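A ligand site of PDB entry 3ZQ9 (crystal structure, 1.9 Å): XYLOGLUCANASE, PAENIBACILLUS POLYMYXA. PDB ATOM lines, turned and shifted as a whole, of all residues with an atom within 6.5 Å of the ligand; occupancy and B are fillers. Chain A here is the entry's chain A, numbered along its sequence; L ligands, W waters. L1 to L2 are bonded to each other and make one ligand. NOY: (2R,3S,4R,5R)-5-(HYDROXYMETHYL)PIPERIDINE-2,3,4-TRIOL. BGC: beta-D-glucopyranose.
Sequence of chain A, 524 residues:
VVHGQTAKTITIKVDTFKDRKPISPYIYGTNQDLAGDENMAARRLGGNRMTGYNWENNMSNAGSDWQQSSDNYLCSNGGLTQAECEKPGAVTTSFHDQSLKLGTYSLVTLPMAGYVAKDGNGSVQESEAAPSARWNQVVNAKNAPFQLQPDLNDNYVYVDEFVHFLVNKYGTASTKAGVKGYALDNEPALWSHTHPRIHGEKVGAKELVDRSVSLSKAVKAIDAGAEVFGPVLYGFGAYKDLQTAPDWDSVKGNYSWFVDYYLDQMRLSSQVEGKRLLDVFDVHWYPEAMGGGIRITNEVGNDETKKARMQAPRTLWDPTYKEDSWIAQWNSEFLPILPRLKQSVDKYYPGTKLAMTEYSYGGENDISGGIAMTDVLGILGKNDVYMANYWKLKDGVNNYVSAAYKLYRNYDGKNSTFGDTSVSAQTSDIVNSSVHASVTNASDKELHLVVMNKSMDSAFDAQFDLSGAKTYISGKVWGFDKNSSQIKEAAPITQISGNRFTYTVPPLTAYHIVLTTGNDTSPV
Water W9 bridges O6 of BGC L2 and O of Gly 46.
Water W4 lies within hydrogen-bond range of an oxygen (O4) of BGC L2 and the side-chain hydroxyl of Tyr 73.
Water W7 lies within hydrogen-bond range of NE of Arg 49 (2.9 Å) and O4 of BGC L2 (2.9 Å).
Water W8 lies within hydrogen-bond range of the side-chain carboxylate of Asp 395 and an oxygen (O3) of BGC L2.
Water W6 bridges the side-chain carboxylate (OD1) of Asp 65 (2.6 Å) and an oxygen (O2) of BGC L2 (3.0 Å).
Water W5 lies within hydrogen-bond range of the backbone carbonyl oxygen (O) of Lys 392 and the indole nitrogen (NE1) of Trp 391.
O6 of BGC L2 is in hydrogen-bond range of N of Arg 49, 3.0 Å away.
The side-chain amide oxygen (OD1) of Asn 186 is in hydrogen-bond range of an oxygen (O2) of NOY L1, 3.0 Å away.
The side-chain amide oxygen (OD1) of Asn 48 lies close to an oxygen (O2) of NOY L1 (3.4 Å).
N of NOY L1 is in salt-bridge range of OE1 of Glu 358 (2.6 Å).
OE2 of Glu 187 lies within salt-bridge range of N of NOY L1, 2.8 Å away.
An oxygen (O4) of NOY L1 lies close to the indole nitrogen (NE1) of Trp 391.
N of Asn 48 sits at hydrogen-bond distance from O3 of NOY L1, at 2.8 Å.
CA of Gly 47 touches O2 of NOY L1, at 3.3 Å.
Asp 65 touches the ligand.
OH of Tyr 286 touches C5 of NOY L1, at 3.8 Å.
CD2 of Leu 393 touches C6 of NOY L1, at 3.7 Å.
Hydrophobic or aromatic side chains within 4 Å of the ligand: Tyr 286, Trp 391 and Leu 393.
NH2 of Arg 44 lies close to ND2 of Asn 186.
OE1 of Glu 358 sits at hydrogen-bond distance from OH of Tyr 286.
The side-chain amide nitrogen (ND2) of Asn 186 lies close to the backbone NH (N) of Gly 47, 3.3 Å away.
OD1 of Asn 186 sits close to OD1 of Asn 48.
The side-chain carboxylate (OE2) of Glu 358 lies within salt-bridge range of the guanidinium group (NH1) of Arg 44 (3.1 Å).
ND1 of His 284 lies within hydrogen-bond range of OE2 of Glu 187, 2.7 Å away.
The side-chain amide nitrogen (ND2) of Asn 48 lies within hydrogen-bond range of the side-chain carboxylate (OD2) of Asp 65, at 2.9 Å.
The side-chain amide nitrogen (NE2) of Gln 32 lies close to the indole nitrogen (NE1) of Trp 391 (3.4 Å).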
ATOM      1  N   GLN A  32     -20.519 -10.785   4.850  1.00  0.00           N
ATOM      2  CA  GLN A  32     -19.474 -11.048   3.819  1.00  0.00           C
ATOM      3  C   GLN A  32     -19.037  -9.762   3.172  1.00  0.00           C
ATOM      4  O   GLN A  32     -19.869  -8.954   2.761  1.00  0.00           O
ATOM      5  CB  GLN A  32     -20.013 -11.970   2.712  1.00  0.00           C
ATOM      6  CG  GLN A  32     -20.565 -13.309   3.231  1.00  0.00           C
ATOM      7  CD  GLN A  32     -22.081 -13.256   3.487  1.00  0.00           C
ATOM      8  OE1 GLN A  32     -22.637 -12.195   3.684  1.00  0.00           O
ATOM      9  NE2 GLN A  32     -22.765 -14.405   3.367  1.00  0.00           N
ATOM     10  N   ARG A  44     -19.347  -7.667  10.339  1.00  0.00           N
ATOM     11  CA  ARG A  44     -19.758  -8.662  11.326  1.00  0.00           C
ATOM     12  C   ARG A  44     -19.154 -10.020  11.008  1.00  0.00           C
ATOM     13  O   ARG A  44     -19.169 -10.466   9.833  1.00  0.00           O
ATOM     14  CB  ARG A  44     -21.294  -8.800  11.327  1.00  0.00           C
ATOM     15  CG  ARG A  44     -21.842 -10.041  12.108  1.00  0.00           C
ATOM     16  CD  ARG A  44     -23.367  -9.879  12.201  1.00  0.00           C
ATOM     17  NE  ARG A  44     -24.065 -10.910  13.004  1.00  0.00           N
ATOM     18  CZ  ARG A  44     -24.644 -12.001  12.513  1.00  0.00           C
ATOM     19  NH1 ARG A  44     -24.499 -12.296  11.206  1.00  0.00           N
ATOM     20  NH2 ARG A  44     -25.332 -12.851  13.335  1.00  0.00           N
ATOM     21  N   GLY A  46     -20.283 -13.466  11.992  1.00  0.00           N
ATOM     22  CA  GLY A  46     -21.518 -13.957  12.661  1.00  0.00           C
ATOM     23  C   GLY A  46     -22.160 -14.983  11.775  1.00  0.00           C
ATOM     24  O   GLY A  46     -21.616 -15.299  10.728  1.00  0.00           O
ATOM     25  N   GLY A  47     -23.305 -15.522  12.201  1.00  0.00           N
ATOM     26  CA  GLY A  47     -24.008 -16.464  11.362  1.00  0.00           C
ATOM     27  C   GLY A  47     -23.804 -17.896  11.866  1.00  0.00           C
ATOM     28  O   GLY A  47     -23.147 -18.124  12.888  1.00  0.00           O
ATOM     29  N   ASN A  48     -24.359 -18.849  11.115  1.00  0.00           N
ATOM     30  CA  ASN A  48     -24.533 -20.234  11.600  1.00  0.00           C
ATOM     31  C   ASN A  48     -23.187 -20.856  11.983  1.00  0.00           C
ATOM     32  O   ASN A  48     -23.056 -21.514  13.015  1.00  0.00           O
ATOM     33  CB  ASN A  48     -25.188 -21.099  10.514  1.00  0.00           C
ATOM     34  CG  ASN A  48     -26.675 -20.792  10.333  1.00  0.00           C
ATOM     35  OD1 ASN A  48     -27.278 -20.120  11.163  1.00  0.00           O
ATOM     36  ND2 ASN A  48     -27.286 -21.339   9.276  1.00  0.00           N
ATOM     37  N   ARG A  49     -22.178 -20.636  11.157  1.00  0.00           N
ATOM     38  CA  ARG A  49     -20.848 -21.195  11.454  1.00  0.00           C
ATOM     39  C   ARG A  49     -20.232 -20.734  12.780  1.00  0.00           C
ATOM     40  O   ARG A  49     -19.354 -21.442  13.340  1.00  0.00           O
ATOM     41  CB  ARG A  49     -19.881 -20.868  10.297  1.00  0.00           C
ATOM     42  CG  ARG A  49     -19.988 -21.841   9.124  1.00  0.00           C
ATOM     43  CD  ARG A  49     -19.234 -23.098   9.420  1.00  0.00           C
ATOM     44  NE  ARG A  49     -19.237 -24.017   8.281  1.00  0.00           N
ATOM     45  CZ  ARG A  49     -18.434 -25.079   8.195  1.00  0.00           C
ATOM     46  NH1 ARG A  49     -17.581 -25.366   9.177  1.00  0.00           N
ATOM     47  NH2 ARG A  49     -18.442 -25.833   7.080  1.00  0.00           N
ATOM     48  N   MET A  50     -20.671 -19.590  13.303  1.00  0.00           N
ATOM     49  CA  MET A  50     -20.008 -19.049  14.504  1.00  0.00           C
ATOM     50  C   MET A  50     -20.489 -19.731  15.831  1.00  0.00           C
ATOM     51  O   MET A  50     -19.786 -19.657  16.849  1.00  0.00           O
ATOM     52  CB  MET A  50     -20.104 -17.517  14.550  1.00  0.00           C
ATOM     53  CG  MET A  50     -19.272 -16.834  13.448  1.00  0.00           C
ATOM     54  SD  MET A  50     -17.514 -17.219  13.636  1.00  0.00           S
ATOM     55  CE  MET A  50     -17.139 -16.425  15.190  1.00  0.00           C
ATOM     56  N   ALA A  62     -20.650 -26.804  10.361  1.00  0.00           N
ATOM     57  CA  ALA A  62     -21.715 -26.286   9.450  1.00  0.00           C
ATOM     58  C   ALA A  62     -23.141 -26.524   9.890  1.00  0.00           C
ATOM     59  O   ALA A  62     -24.044 -25.869   9.398  1.00  0.00           O
ATOM     60  CB  ALA A  62     -21.527 -26.914   8.023  1.00  0.00           C
ATOM     61  N   ASP A  65     -26.476 -26.837   7.434  1.00  0.00           N
ATOM     62  CA  ASP A  65     -26.085 -26.243   6.158  1.00  0.00           C
ATOM     63  C   ASP A  65     -25.213 -27.192   5.352  1.00  0.00           C
ATOM     64  O   ASP A  65     -25.231 -27.160   4.100  1.00  0.00           O
ATOM     65  CB  ASP A  65     -25.329 -24.921   6.336  1.00  0.00           C
ATOM     66  CG  ASP A  65     -26.267 -23.748   6.697  1.00  0.00           C
ATOM     67  OD1 ASP A  65     -27.493 -23.794   6.384  1.00  0.00           O
ATOM     68  OD2 ASP A  65     -25.756 -22.790   7.284  1.00  0.00           O
ATOM     69  N   TYR A  73     -13.623 -24.531   7.410  1.00  0.00           N
ATOM     70  CA  TYR A  73     -14.278 -23.591   6.502  1.00  0.00           C
ATOM     71  C   TYR A  73     -13.980 -22.107   6.828  1.00  0.00           C
ATOM     72  O   TYR A  73     -13.758 -21.305   5.928  1.00  0.00           O
ATOM     73  CB  TYR A  73     -15.787 -23.779   6.561  1.00  0.00           C
ATOM     74  CG  TYR A  73     -16.526 -22.669   5.817  1.00  0.00           C
ATOM     75  CD1 TYR A  73     -16.446 -22.592   4.422  1.00  0.00           C
ATOM     76  CD2 TYR A  73     -17.177 -21.648   6.512  1.00  0.00           C
ATOM     77  CE1 TYR A  73     -17.114 -21.559   3.713  1.00  0.00           C
ATOM     78  CE2 TYR A  73     -17.848 -20.629   5.814  1.00  0.00           C
ATOM     79  CZ  TYR A  73     -17.791 -20.602   4.432  1.00  0.00           C
ATOM     80  OH  TYR A  73     -18.402 -19.595   3.706  1.00  0.00           O
ATOM     81  N   LEU A  74     -13.990 -21.753   8.116  1.00  0.00           N
ATOM     82  CA  LEU A  74     -13.836 -20.315   8.444  1.00  0.00           C
ATOM     83  C   LEU A  74     -12.399 -19.831   8.142  1.00  0.00           C
ATOM     84  O   LEU A  74     -12.189 -18.641   7.869  1.00  0.00           O
ATOM     85  CB  LEU A  74     -14.198 -20.093   9.941  1.00  0.00           C
ATOM     86  CG  LEU A  74     -15.695 -20.128  10.231  1.00  0.00           C
ATOM     87  CD1 LEU A  74     -15.943 -19.938  11.759  1.00  0.00           C
ATOM     88  CD2 LEU A  74     -16.525 -19.053   9.403  1.00  0.00           C
ATOM     89  N   ASN A 186     -25.921 -16.925  17.766  1.00  0.00           N
ATOM     90  CA  ASN A 186     -26.603 -16.626  16.488  1.00  0.00           C
ATOM     91  C   ASN A 186     -27.883 -17.460  16.437  1.00  0.00           C
ATOM     92  O   ASN A 186     -27.820 -18.688  16.582  1.00  0.00           O
ATOM     93  CB  ASN A 186     -25.667 -17.063  15.326  1.00  0.00           C
ATOM     94  CG  ASN A 186     -26.298 -16.817  13.964  1.00  0.00           C
ATOM     95  OD1 ASN A 186     -26.771 -17.795  13.263  1.00  0.00           O
ATOM     96  ND2 ASN A 186     -26.351 -15.585  13.570  1.00  0.00           N
ATOM     97  N   GLU A 187     -29.024 -16.799  16.265  1.00  0.00           N
ATOM     98  CA  GLU A 187     -30.308 -17.488  15.964  1.00  0.00           C
ATOM     99  C   GLU A 187     -30.595 -18.674  16.928  1.00  0.00           C
ATOM    100  O   GLU A 187     -30.794 -19.811  16.489  1.00  0.00           O
ATOM    101  CB  GLU A 187     -30.376 -17.947  14.491  1.00  0.00           C
ATOM    102  CG  GLU A 187     -30.165 -16.745  13.536  1.00  0.00           C
ATOM    103  CD  GLU A 187     -30.393 -17.062  12.040  1.00  0.00           C
ATOM    104  OE1 GLU A 187     -30.500 -18.250  11.667  1.00  0.00           O
ATOM    105  OE2 GLU A 187     -30.483 -16.063  11.232  1.00  0.00           O
ATOM    106  N   TYR A 234     -33.688 -14.946  14.434  1.00  0.00           N
ATOM    107  CA  TYR A 234     -33.611 -15.242  12.998  1.00  0.00           C
ATOM    108  C   TYR A 234     -34.675 -14.510  12.188  1.00  0.00           C
ATOM    109  O   TYR A 234     -34.500 -14.246  11.004  1.00  0.00           O
ATOM    110  CB  TYR A 234     -33.716 -16.783  12.762  1.00  0.00           C
ATOM    111  CG  TYR A 234     -35.117 -17.275  12.653  1.00  0.00           C
ATOM    112  CD1 TYR A 234     -35.769 -17.314  11.392  1.00  0.00           C
ATOM    113  CD2 TYR A 234     -35.824 -17.698  13.778  1.00  0.00           C
ATOM    114  CE1 TYR A 234     -37.101 -17.743  11.289  1.00  0.00           C
ATOM    115  CE2 TYR A 234     -37.156 -18.163  13.666  1.00  0.00           C
ATOM    116  CZ  TYR A 234     -37.778 -18.178  12.418  1.00  0.00           C
ATOM    117  OH  TYR A 234     -39.082 -18.593  12.283  1.00  0.00           O
ATOM    118  N   HIS A 284     -32.338 -10.430  12.902  1.00  0.00           N
ATOM    119  CA  HIS A 284     -32.170 -10.677  11.461  1.00  0.00           C
ATOM    120  C   HIS A 284     -33.539 -10.505  10.789  1.00  0.00           C
ATOM    121  O   HIS A 284     -34.563 -10.836  11.382  1.00  0.00           O
ATOM    122  CB  HIS A 284     -31.687 -12.126  11.279  1.00  0.00           C
ATOM    123  CG  HIS A 284     -30.329 -12.349  11.850  1.00  0.00           C
ATOM    124  ND1 HIS A 284     -29.747 -13.590  11.968  1.00  0.00           N
ATOM    125  CD2 HIS A 284     -29.450 -11.465  12.398  1.00  0.00           C
ATOM    126  CE1 HIS A 284     -28.554 -13.464  12.526  1.00  0.00           C
ATOM    127  NE2 HIS A 284     -28.342 -12.177  12.777  1.00  0.00           N
ATOM    128  N   TYR A 286     -35.281 -11.105   7.079  1.00  0.00           N
ATOM    129  CA  TYR A 286     -35.339 -11.465   5.683  1.00  0.00           C
ATOM    130  C   TYR A 286     -36.807 -11.357   5.299  1.00  0.00           C
ATOM    131  O   TYR A 286     -37.636 -12.077   5.831  1.00  0.00           O
ATOM    132  CB  TYR A 286     -34.871 -12.888   5.493  1.00  0.00           C
ATOM    133  CG  TYR A 286     -33.379 -13.020   5.725  1.00  0.00           C
ATOM    134  CD1 TYR A 286     -32.486 -12.645   4.719  1.00  0.00           C
ATOM    135  CD2 TYR A 286     -32.876 -13.545   6.920  1.00  0.00           C
ATOM    136  CE1 TYR A 286     -31.109 -12.789   4.899  1.00  0.00           C
ATOM    137  CE2 TYR A 286     -31.492 -13.651   7.124  1.00  0.00           C
ATOM    138  CZ  TYR A 286     -30.614 -13.308   6.091  1.00  0.00           C
ATOM    139  OH  TYR A 286     -29.248 -13.462   6.244  1.00  0.00           O
ATOM    140  N   GLU A 358     -28.395  -9.167  10.056  1.00  0.00           N
ATOM    141  CA  GLU A 358     -28.496  -9.815   8.740  1.00  0.00           C
ATOM    142  C   GLU A 358     -29.799  -9.344   8.108  1.00  0.00           C
ATOM    143  O   GLU A 358     -30.808  -9.267   8.811  1.00  0.00           O
ATOM    144  CB  GLU A 358     -28.569 -11.334   8.859  1.00  0.00           C
ATOM    145  CG  GLU A 358     -27.246 -12.038   9.312  1.00  0.00           C
ATOM    146  CD  GLU A 358     -27.407 -13.560   9.369  1.00  0.00           C
ATOM    147  OE1 GLU A 358     -28.285 -14.103   8.631  1.00  0.00           O
ATOM    148  OE2 GLU A 358     -26.669 -14.219  10.160  1.00  0.00           O
ATOM    149  N   TRP A 391     -26.512  -9.571   4.366  1.00  0.00           N
ATOM    150  CA  TRP A 391     -26.024 -10.977   4.284  1.00  0.00           C
ATOM    151  C   TRP A 391     -26.234 -11.474   2.825  1.00  0.00           C
ATOM    152  O   TRP A 391     -27.326 -11.355   2.314  1.00  0.00           O
ATOM    153  CB  TRP A 391     -26.807 -11.894   5.264  1.00  0.00           C
ATOM    154  CG  TRP A 391     -26.267 -13.294   5.204  1.00  0.00           C
ATOM    155  CD1 TRP A 391     -26.610 -14.251   4.276  1.00  0.00           C
ATOM    156  CD2 TRP A 391     -25.296 -13.880   6.065  1.00  0.00           C
ATOM    157  NE1 TRP A 391     -25.872 -15.395   4.493  1.00  0.00           N
ATOM    158  CE2 TRP A 391     -25.052 -15.185   5.582  1.00  0.00           C
ATOM    159  CE3 TRP A 391     -24.589 -13.427   7.191  1.00  0.00           C
ATOM    160  CZ2 TRP A 391     -24.129 -16.071   6.191  1.00  0.00           C
ATOM    161  CZ3 TRP A 391     -23.661 -14.305   7.803  1.00  0.00           C
ATOM    162  CH2 TRP A 391     -23.418 -15.599   7.285  1.00  0.00           C
ATOM    163  N   LYS A 392     -25.184 -11.976   2.190  1.00  0.00           N
ATOM    164  CA  LYS A 392     -25.270 -12.478   0.821  1.00  0.00           C
ATOM    165  C   LYS A 392     -26.042 -13.800   0.767  1.00  0.00           C
ATOM    166  O   LYS A 392     -25.500 -14.838   1.167  1.00  0.00           O
ATOM    167  CB  LYS A 392     -23.841 -12.758   0.294  1.00  0.00           C
ATOM    168  CG  LYS A 392     -22.943 -11.533   0.178  1.00  0.00           C
ATOM    169  CD  LYS A 392     -21.563 -11.975  -0.376  1.00  0.00           C
ATOM    170  CE  LYS A 392     -21.650 -12.315  -1.851  1.00  0.00           C
ATOM    171  NZ  LYS A 392     -20.258 -12.853  -2.285  1.00  0.00           N
ATOM    172  N   LEU A 393     -27.263 -13.787   0.202  1.00  0.00           N
ATOM    173  CA  LEU A 393     -28.010 -15.016   0.035  1.00  0.00           C
ATOM    174  C   LEU A 393     -27.599 -15.709  -1.265  1.00  0.00           C
ATOM    175  O   LEU A 393     -27.922 -16.874  -1.473  1.00  0.00           O
ATOM    176  CB  LEU A 393     -29.514 -14.744  -0.032  1.00  0.00           C
ATOM    177  CG  LEU A 393     -30.118 -14.242   1.278  1.00  0.00           C
ATOM    178  CD1 LEU A 393     -31.566 -13.894   1.035  1.00  0.00           C
ATOM    179  CD2 LEU A 393     -29.949 -15.295   2.409  1.00  0.00           C
ATOM    180  N   ASP A 395     -24.214 -16.529  -3.641  1.00  0.00           N
ATOM    181  CA  ASP A 395     -22.734 -16.530  -3.640  1.00  0.00           C
ATOM    182  C   ASP A 395     -22.226 -15.840  -4.889  1.00  0.00           C
ATOM    183  O   ASP A 395     -22.991 -15.644  -5.837  1.00  0.00           O
ATOM    184  CB  ASP A 395     -22.187 -17.971  -3.584  1.00  0.00           C
ATOM    185  CG  ASP A 395     -22.580 -18.704  -2.270  1.00  0.00           C
ATOM    186  OD1 ASP A 395     -22.550 -18.080  -1.206  1.00  0.00           O
ATOM    187  OD2 ASP A 395     -22.855 -19.930  -2.310  1.00  0.00           O
HETATM  188  O4  NOY L   1     -26.518 -18.296   5.882  1.00  0.00           O
HETATM  189  C4  NOY L   1     -27.451 -18.149   6.969  1.00  0.00           C
HETATM  190  C3  NOY L   1     -26.768 -17.500   8.186  1.00  0.00           C
HETATM  191  O3  NOY L   1     -25.679 -18.277   8.658  1.00  0.00           O
HETATM  192  C2  NOY L   1     -27.809 -17.350   9.323  1.00  0.00           C
HETATM  193  N   NOY L   1     -28.990 -16.569   8.897  1.00  0.00           N
HETATM  194  C7  NOY L   1     -29.630 -17.061   7.650  1.00  0.00           C
HETATM  195  C5  NOY L   1     -28.566 -17.186   6.544  1.00  0.00           C
HETATM  196  C6  NOY L   1     -29.190 -17.570   5.200  1.00  0.00           C
HETATM  197  O2  NOY L   1     -27.218 -16.754  10.478  1.00  0.00           O
HETATM  198  O6  NOY L   1     -29.947 -18.778   5.325  1.00  0.00           O
HETATM  199  C2  BGC L   2     -25.587 -19.894   4.339  1.00  0.00           C
HETATM  200  C3  BGC L   2     -24.584 -21.033   4.259  1.00  0.00           C
HETATM  201  C4  BGC L   2     -23.292 -20.569   4.946  1.00  0.00           C
HETATM  202  C5  BGC L   2     -23.525 -20.218   6.419  1.00  0.00           C
HETATM  203  C6  BGC L   2     -22.243 -19.667   7.055  1.00  0.00           C
HETATM  204  C1  BGC L   2     -25.740 -19.487   5.812  1.00  0.00           C
HETATM  205  O2  BGC L   2     -26.881 -20.306   3.956  1.00  0.00           O
HETATM  206  O3  BGC L   2     -24.301 -21.289   2.859  1.00  0.00           O
HETATM  207  O4  BGC L   2     -22.265 -21.542   4.771  1.00  0.00           O
HETATM  208  O5  BGC L   2     -24.520 -19.177   6.419  1.00  0.00           O
HETATM  209  O6  BGC L   2     -22.493 -19.361   8.423  1.00  0.00           O
HETATM  210  O   HOH W   1     -31.565 -19.208   9.400  1.00  0.00           O
HETATM  211  O   HOH W   2     -25.406 -23.683   2.315  1.00  0.00           O
HETATM  212  O   HOH W   3     -30.431 -19.705   2.694  1.00  0.00           O
HETATM  213  O   HOH W   4     -20.779 -21.512   2.565  1.00  0.00           O
HETATM  214  O   HOH W   5     -25.800 -17.297   2.144  1.00  0.00           O
HETATM  215  O   HOH W   6     -28.843 -21.590   5.866  1.00  0.00           O
HETATM  216  O   HOH W   7     -21.616 -23.668   6.660  1.00  0.00           O
HETATM  217  O   HOH W   8     -23.438 -18.842   1.445  1.00  0.00           O
HETATM  218  O   HOH W   9     -20.796 -17.530   9.292  1.00  0.00           O
